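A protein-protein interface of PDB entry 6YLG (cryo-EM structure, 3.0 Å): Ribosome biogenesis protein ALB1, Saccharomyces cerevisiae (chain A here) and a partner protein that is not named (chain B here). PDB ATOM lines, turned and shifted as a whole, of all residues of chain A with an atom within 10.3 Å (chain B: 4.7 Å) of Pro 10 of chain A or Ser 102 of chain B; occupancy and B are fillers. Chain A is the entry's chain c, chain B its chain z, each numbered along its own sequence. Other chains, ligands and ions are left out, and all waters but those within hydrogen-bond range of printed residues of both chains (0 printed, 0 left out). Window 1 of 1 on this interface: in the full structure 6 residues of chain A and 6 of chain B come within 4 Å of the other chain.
The backbone carbonyl oxygen of Gln 96 of chain B is in hydrogen-bond range of the backbone NH of Thr 101 of chain B (3.0 Å).
OE1 of Gln 96 of chain B is in hydrogen-bond range of OG of Ser 102 of chain B.
The backbone NH (N) of Arg 105 of chain B lies within hydrogen-bond range of the side-chain hydroxyl (OG) of Ser 102 of chain B (3.2 Å).
Of the printed residues of chain B, Ser 6 of chain A touches Phe 103 (3.7 Å).
Of the printed residues of chain B, Asn 8 of chain A touches Ser 102 (3.5 Å) and Phe 103 (2.7 Å).
Of the printed residues of chain B, Pro 10 of chain A touches Lys 100 (3.4 Å) and Ser 102 (3.7 Å).
Thr 13 of chain A touches none of the printed residues of chain B.
Thr 101 of chain B touches one residue of chain A.
Printed residues of chain A within 4 Å of Ser 102 of chain B: Asn 8 and Pro 10.
No residue of chain A comes within 4 Å of Thr 104 of chain B.
The nearest residue of chain A that does not touch Ser 102 of chain B is Arg 9 of chain A (4.2 Å).
Hydrophobic or aromatic side chains of chain A that line the printed part of chain B: Pro 10.
Hydrophobic or aromatic side chains of chain B that line the printed part of chain A: Phe 103.
Among the printed residues, no Asp or Glu carboxylate lies within 4 Å of a Lys or Arg side-chain nitrogen of the other chain.
Among the printed residues, pairs that only touch across the chains: Ser 14 of chain A with Thr 101 of chain B, Pro 10 of chain A with Lys 100 of chain B, Ser 6 of chain A with Phe 103 of chain B, Pro 10 of chain A with Ser 102 of chain B and Arg 9 of chain A with Phe 103 of chain B.
O of Asn 8 of chain A lies close to O of Phe 103 of chain B (2.7 Å).
The backbone carbonyl oxygen (O) of Ser 102 of chain B sits close to the backbone carbonyl oxygen (O) of Asn 8 of chain A (3.5 Å).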
ATOM      1  N   SER A   3      12.315  -2.619 -11.062  1.00  0.00           N
ATOM      2  CA  SER A   3      12.259  -1.182 -10.813  1.00  0.00           C
ATOM      3  C   SER A   3      11.514  -0.414 -11.905  1.00  0.00           C
ATOM      4  O   SER A   3      11.394   0.808 -11.827  1.00  0.00           O
ATOM      5  CB  SER A   3      13.675  -0.621 -10.670  1.00  0.00           C
ATOM      6  OG  SER A   3      13.646   0.726 -10.230  1.00  0.00           O
ATOM      7  N   LYS A   4      11.016  -1.121 -12.923  1.00  0.00           N
ATOM      8  CA  LYS A   4      10.235  -0.486 -13.976  1.00  0.00           C
ATOM      9  C   LYS A   4       8.771  -0.316 -13.601  1.00  0.00           C
ATOM     10  O   LYS A   4       8.157   0.683 -13.988  1.00  0.00           O
ATOM     11  CB  LYS A   4      10.329  -1.296 -15.275  1.00  0.00           C
ATOM     12  CG  LYS A   4       9.754  -2.698 -15.200  1.00  0.00           C
ATOM     13  CD  LYS A   4      10.015  -3.461 -16.482  1.00  0.00           C
ATOM     14  CE  LYS A   4       9.234  -4.761 -16.519  1.00  0.00           C
ATOM     15  NZ  LYS A   4       9.791  -5.759 -15.573  1.00  0.00           N
ATOM     16  N   ASN A   5       8.204  -1.268 -12.861  1.00  0.00           N
ATOM     17  CA  ASN A   5       6.818  -1.156 -12.431  1.00  0.00           C
ATOM     18  C   ASN A   5       6.640  -0.088 -11.362  1.00  0.00           C
ATOM     19  O   ASN A   5       5.540   0.454 -11.212  1.00  0.00           O
ATOM     20  CB  ASN A   5       6.333  -2.506 -11.912  1.00  0.00           C
ATOM     21  CG  ASN A   5       6.416  -3.593 -12.957  1.00  0.00           C
ATOM     22  OD1 ASN A   5       6.070  -3.383 -14.120  1.00  0.00           O
ATOM     23  ND2 ASN A   5       6.880  -4.765 -12.552  1.00  0.00           N
ATOM     24  N   SER A   6       7.701   0.221 -10.616  1.00  0.00           N
ATOM     25  CA  SER A   6       7.723   1.267  -9.593  1.00  0.00           C
ATOM     26  C   SER A   6       9.037   2.021  -9.779  1.00  0.00           C
ATOM     27  O   SER A   6      10.056   1.666  -9.184  1.00  0.00           O
ATOM     28  CB  SER A   6       7.596   0.683  -8.196  1.00  0.00           C
ATOM     29  OG  SER A   6       8.679  -0.185  -7.912  1.00  0.00           O
ATOM     30  N   ILE A   7       9.053   3.042 -10.638  1.00  0.00           N
ATOM     31  CA  ILE A   7      10.297   3.757 -10.909  1.00  0.00           C
ATOM     32  C   ILE A   7      10.584   4.819  -9.859  1.00  0.00           C
ATOM     33  O   ILE A   7      11.753   5.147  -9.626  1.00  0.00           O
ATOM     34  CB  ILE A   7      10.294   4.398 -12.310  1.00  0.00           C
ATOM     35  CG1 ILE A   7       9.068   5.290 -12.543  1.00  0.00           C
ATOM     36  CG2 ILE A   7      10.347   3.325 -13.381  1.00  0.00           C
ATOM     37  CD1 ILE A   7       9.340   6.459 -13.462  1.00  0.00           C
ATOM     38  N   ASN A   8       9.551   5.363  -9.219  1.00  0.00           N
ATOM     39  CA  ASN A   8       9.706   6.391  -8.204  1.00  0.00           C
ATOM     40  C   ASN A   8       9.855   5.820  -6.798  1.00  0.00           C
ATOM     41  O   ASN A   8       9.770   6.578  -5.826  1.00  0.00           O
ATOM     42  CB  ASN A   8       8.517   7.348  -8.261  1.00  0.00           C
ATOM     43  CG  ASN A   8       8.435   8.088  -9.580  1.00  0.00           C
ATOM     44  OD1 ASN A   8       9.413   8.164 -10.321  1.00  0.00           O
ATOM     45  ND2 ASN A   8       7.268   8.633  -9.882  1.00  0.00           N
ATOM     46  N   ARG A   9      10.080   4.511  -6.669  1.00  0.00           N
ATOM     47  CA  ARG A   9      10.339   3.856  -5.401  1.00  0.00           C
ATOM     48  C   ARG A   9      11.786   3.375  -5.364  1.00  0.00           C
ATOM     49  O   ARG A   9      12.190   2.610  -6.252  1.00  0.00           O
ATOM     50  CB  ARG A   9       9.405   2.664  -5.196  1.00  0.00           C
ATOM     51  CG  ARG A   9       9.574   1.996  -3.842  1.00  0.00           C
ATOM     52  CD  ARG A   9       8.460   1.021  -3.544  1.00  0.00           C
ATOM     53  NE  ARG A   9       8.546  -0.178  -4.370  1.00  0.00           N
ATOM     54  CZ  ARG A   9       7.658  -1.168  -4.361  1.00  0.00           C
ATOM     55  NH1 ARG A   9       6.595  -1.126  -3.568  1.00  0.00           N
ATOM     56  NH2 ARG A   9       7.835  -2.216  -5.154  1.00  0.00           N
ATOM     57  N   PRO A  10      12.596   3.780  -4.383  1.00  0.00           N
ATOM     58  CA  PRO A  10      13.931   3.184  -4.268  1.00  0.00           C
ATOM     59  C   PRO A  10      13.864   1.706  -3.923  1.00  0.00           C
ATOM     60  O   PRO A  10      13.030   1.269  -3.128  1.00  0.00           O
ATOM     61  CB  PRO A  10      14.584   3.994  -3.146  1.00  0.00           C
ATOM     62  CG  PRO A  10      13.914   5.296  -3.214  1.00  0.00           C
ATOM     63  CD  PRO A  10      12.487   4.973  -3.525  1.00  0.00           C
ATOM     64  N   LYS A  11      14.755   0.940  -4.547  1.00  0.00           N
ATOM     65  CA  LYS A  11      14.875  -0.500  -4.352  1.00  0.00           C
ATOM     66  C   LYS A  11      16.224  -0.895  -3.779  1.00  0.00           C
ATOM     67  O   LYS A  11      16.294  -1.505  -2.699  1.00  0.00           O
ATOM     68  CB  LYS A  11      14.652  -1.195  -5.706  1.00  0.00           C
ATOM     69  CG  LYS A  11      14.175  -2.625  -5.642  1.00  0.00           C
ATOM     70  CD  LYS A  11      13.960  -3.162  -7.049  1.00  0.00           C
ATOM     71  CE  LYS A  11      13.067  -4.380  -7.065  1.00  0.00           C
ATOM     72  NZ  LYS A  11      13.722  -5.549  -6.440  1.00  0.00           N
ATOM     73  N   LEU A  12      17.311  -0.513  -4.449  1.00  0.00           N
ATOM     74  CA  LEU A  12      18.635  -0.979  -4.066  1.00  0.00           C
ATOM     75  C   LEU A  12      19.137  -0.272  -2.817  1.00  0.00           C
ATOM     76  O   LEU A  12      19.765  -0.902  -1.960  1.00  0.00           O
ATOM     77  CB  LEU A  12      19.612  -0.776  -5.222  1.00  0.00           C
ATOM     78  CG  LEU A  12      20.926  -1.554  -5.135  1.00  0.00           C
ATOM     79  CD1 LEU A  12      20.736  -3.030  -5.461  1.00  0.00           C
ATOM     80  CD2 LEU A  12      21.943  -0.932  -6.065  1.00  0.00           C
ATOM     81  N   THR A  13      18.894   1.034  -2.703  1.00  0.00           N
ATOM     82  CA  THR A  13      19.290   1.745  -1.493  1.00  0.00           C
ATOM     83  C   THR A  13      18.595   1.176  -0.263  1.00  0.00           C
ATOM     84  O   THR A  13      19.222   1.037   0.794  1.00  0.00           O
ATOM     85  CB  THR A  13      18.990   3.237  -1.638  1.00  0.00           C
ATOM     86  OG1 THR A  13      17.647   3.418  -2.101  1.00  0.00           O
ATOM     87  CG2 THR A  13      19.949   3.883  -2.628  1.00  0.00           C
ATOM     88  N   SER A  14      17.321   0.803  -0.390  1.00  0.00           N
ATOM     89  CA  SER A  14      16.613   0.171   0.715  1.00  0.00           C
ATOM     90  C   SER A  14      17.189  -1.201   1.032  1.00  0.00           C
ATOM     91  O   SER A  14      17.386  -1.538   2.207  1.00  0.00           O
ATOM     92  CB  SER A  14      15.129   0.056   0.384  1.00  0.00           C
ATOM     93  OG  SER A  14      14.455  -0.732   1.348  1.00  0.00           O
ATOM     94  N   ASN A  15      17.446  -2.012   0.000  1.00  0.00           N
ATOM     95  CA  ASN A  15      18.055  -3.320   0.224  1.00  0.00           C
ATOM     96  C   ASN A  15      19.397  -3.206   0.939  1.00  0.00           C
ATOM     97  O   ASN A  15      19.698  -4.008   1.832  1.00  0.00           O
ATOM     98  CB  ASN A  15      18.230  -4.043  -1.106  1.00  0.00           C
ATOM     99  CG  ASN A  15      16.909  -4.405  -1.748  1.00  0.00           C
ATOM    100  OD1 ASN A  15      15.847  -3.990  -1.286  1.00  0.00           O
ATOM    101  ND2 ASN A  15      16.967  -5.187  -2.821  1.00  0.00           N
ATOM    102  N   LEU A  16      20.200  -2.204   0.585  1.00  0.00           N
ATOM    103  CA  LEU A  16      21.516  -2.061   1.195  1.00  0.00           C
ATOM    104  C   LEU A  16      21.433  -1.502   2.607  1.00  0.00           C
ATOM    105  O   LEU A  16      22.220  -1.908   3.469  1.00  0.00           O
ATOM    106  CB  LEU A  16      22.400  -1.173   0.318  1.00  0.00           C
ATOM    107  CG  LEU A  16      22.768  -1.731  -1.065  1.00  0.00           C
ATOM    108  CD1 LEU A  16      23.585  -0.726  -1.851  1.00  0.00           C
ATOM    109  CD2 LEU A  16      23.519  -3.052  -0.971  1.00  0.00           C
ATOM    110  N   HIS A  17      20.512  -0.567   2.858  1.00  0.00           N
ATOM    111  CA  HIS A  17      20.192  -0.170   4.226  1.00  0.00           C
ATOM    112  C   HIS A  17      19.843  -1.380   5.085  1.00  0.00           C
ATOM    113  O   HIS A  17      20.365  -1.539   6.202  1.00  0.00           O
ATOM    114  CB  HIS A  17      19.027   0.818   4.193  1.00  0.00           C
ATOM    115  CG  HIS A  17      18.779   1.517   5.489  1.00  0.00           C
ATOM    116  ND1 HIS A  17      17.766   1.156   6.351  1.00  0.00           N
ATOM    117  CD2 HIS A  17      19.396   2.577   6.058  1.00  0.00           C
ATOM    118  CE1 HIS A  17      17.782   1.954   7.404  1.00  0.00           C
ATOM    119  NE2 HIS A  17      18.762   2.825   7.250  1.00  0.00           N
ATOM    120  N   GLN B  96       7.785   3.463   5.798  1.00  0.00           N
ATOM    121  CA  GLN B  96       8.211   3.907   4.479  1.00  0.00           C
ATOM    122  C   GLN B  96       9.405   4.846   4.532  1.00  0.00           C
ATOM    123  O   GLN B  96      10.311   4.715   3.707  1.00  0.00           O
ATOM    124  CB  GLN B  96       7.061   4.617   3.764  1.00  0.00           C
ATOM    125  CG  GLN B  96       6.028   3.696   3.151  1.00  0.00           C
ATOM    126  CD  GLN B  96       5.110   4.421   2.189  1.00  0.00           C
ATOM    127  OE1 GLN B  96       5.162   5.646   2.067  1.00  0.00           O
ATOM    128  NE2 GLN B  96       4.266   3.669   1.496  1.00  0.00           N
ATOM    129  N   LYS B 100      13.015   3.839   3.412  1.00  0.00           N
ATOM    130  CA  LYS B 100      13.170   4.636   2.198  1.00  0.00           C
ATOM    131  C   LYS B 100      12.369   4.073   1.025  1.00  0.00           C
ATOM    132  O   LYS B 100      12.687   4.351  -0.135  1.00  0.00           O
ATOM    133  CB  LYS B 100      14.651   4.771   1.828  1.00  0.00           C
ATOM    134  CG  LYS B 100      15.479   5.402   2.945  1.00  0.00           C
ATOM    135  CD  LYS B 100      16.949   5.530   2.580  1.00  0.00           C
ATOM    136  CE  LYS B 100      17.661   6.550   3.464  1.00  0.00           C
ATOM    137  NZ  LYS B 100      18.942   7.036   2.876  1.00  0.00           N
ATOM    138  N   THR B 101      11.334   3.287   1.312  1.00  0.00           N
ATOM    139  CA  THR B 101      10.467   2.697   0.289  1.00  0.00           C
ATOM    140  C   THR B 101       9.194   3.525   0.110  1.00  0.00           C
ATOM    141  O   THR B 101       8.079   3.028   0.272  1.00  0.00           O
ATOM    142  CB  THR B 101      10.130   1.255   0.656  1.00  0.00           C
ATOM    143  OG1 THR B 101       9.658   1.203   2.009  1.00  0.00           O
ATOM    144  CG2 THR B 101      11.355   0.359   0.516  1.00  0.00           C
ATOM    145  N   SER B 102       9.368   4.800  -0.235  1.00  0.00           N
ATOM    146  CA  SER B 102       8.197   5.620  -0.521  1.00  0.00           C
ATOM    147  C   SER B 102       8.281   6.174  -1.935  1.00  0.00           C
ATOM    148  O   SER B 102       9.337   6.642  -2.370  1.00  0.00           O
ATOM    149  CB  SER B 102       8.066   6.768   0.479  1.00  0.00           C
ATOM    150  OG  SER B 102       7.104   7.708   0.040  1.00  0.00           O
ATOM    151  N   PHE B 103       7.100   6.187  -2.555  1.00  0.00           N
ATOM    152  CA  PHE B 103       6.997   6.614  -3.945  1.00  0.00           C
ATOM    153  C   PHE B 103       7.261   8.105  -4.087  1.00  0.00           C
ATOM    154  O   PHE B 103       8.056   8.522  -4.937  1.00  0.00           O
ATOM    155  CB  PHE B 103       5.614   6.276  -4.495  1.00  0.00           C
ATOM    156  CG  PHE B 103       5.462   4.847  -4.917  1.00  0.00           C
ATOM    157  CD1 PHE B 103       5.240   3.858  -3.981  1.00  0.00           C
ATOM    158  CD2 PHE B 103       5.539   4.494  -6.250  1.00  0.00           C
ATOM    159  CE1 PHE B 103       5.096   2.546  -4.365  1.00  0.00           C
ATOM    160  CE2 PHE B 103       5.399   3.182  -6.639  1.00  0.00           C
ATOM    161  CZ  PHE B 103       5.180   2.207  -5.697  1.00  0.00           C
ATOM    162  N   THR B 104       6.604   8.924  -3.267  1.00  0.00           N
ATOM    163  CA  THR B 104       6.720  10.373  -3.338  1.00  0.00           C
ATOM    164  C   THR B 104       7.827  10.939  -2.468  1.00  0.00           C
ATOM    165  O   THR B 104       8.586  11.790  -2.935  1.00  0.00           O
ATOM    166  CB  THR B 104       5.399  11.034  -2.927  1.00  0.00           C
ATOM    167  OG1 THR B 104       4.939  10.466  -1.694  1.00  0.00           O
ATOM    168  CG2 THR B 104       4.345  10.833  -3.997  1.00  0.00           C
ATOM    169  N   ARG B 105       7.936  10.495  -1.221  1.00  0.00           N
ATOM    170  CA  ARG B 105       8.970  10.976  -0.321  1.00  0.00           C
ATOM    171  C   ARG B 105      10.261  10.206  -0.548  1.00  0.00           C
ATOM    172  O   ARG B 105      10.252   9.042  -0.954  1.00  0.00           O
ATOM    173  CB  ARG B 105       8.531  10.836   1.138  1.00  0.00           C
ATOM    174  CG  ARG B 105       7.103  11.287   1.419  1.00  0.00           C
ATOM    175  CD  ARG B 105       6.799  12.642   0.812  1.00  0.00           C
ATOM    176  NE  ARG B 105       5.655  13.286   1.457  1.00  0.00           N
ATOM    177  CZ  ARG B 105       5.706  13.982   2.591  1.00  0.00           C
ATOM    178  NH1 ARG B 105       6.847  14.146   3.254  1.00  0.00           N
ATOM    179  NH2 ARG B 105       4.595  14.520   3.073  1.00  0.00           N
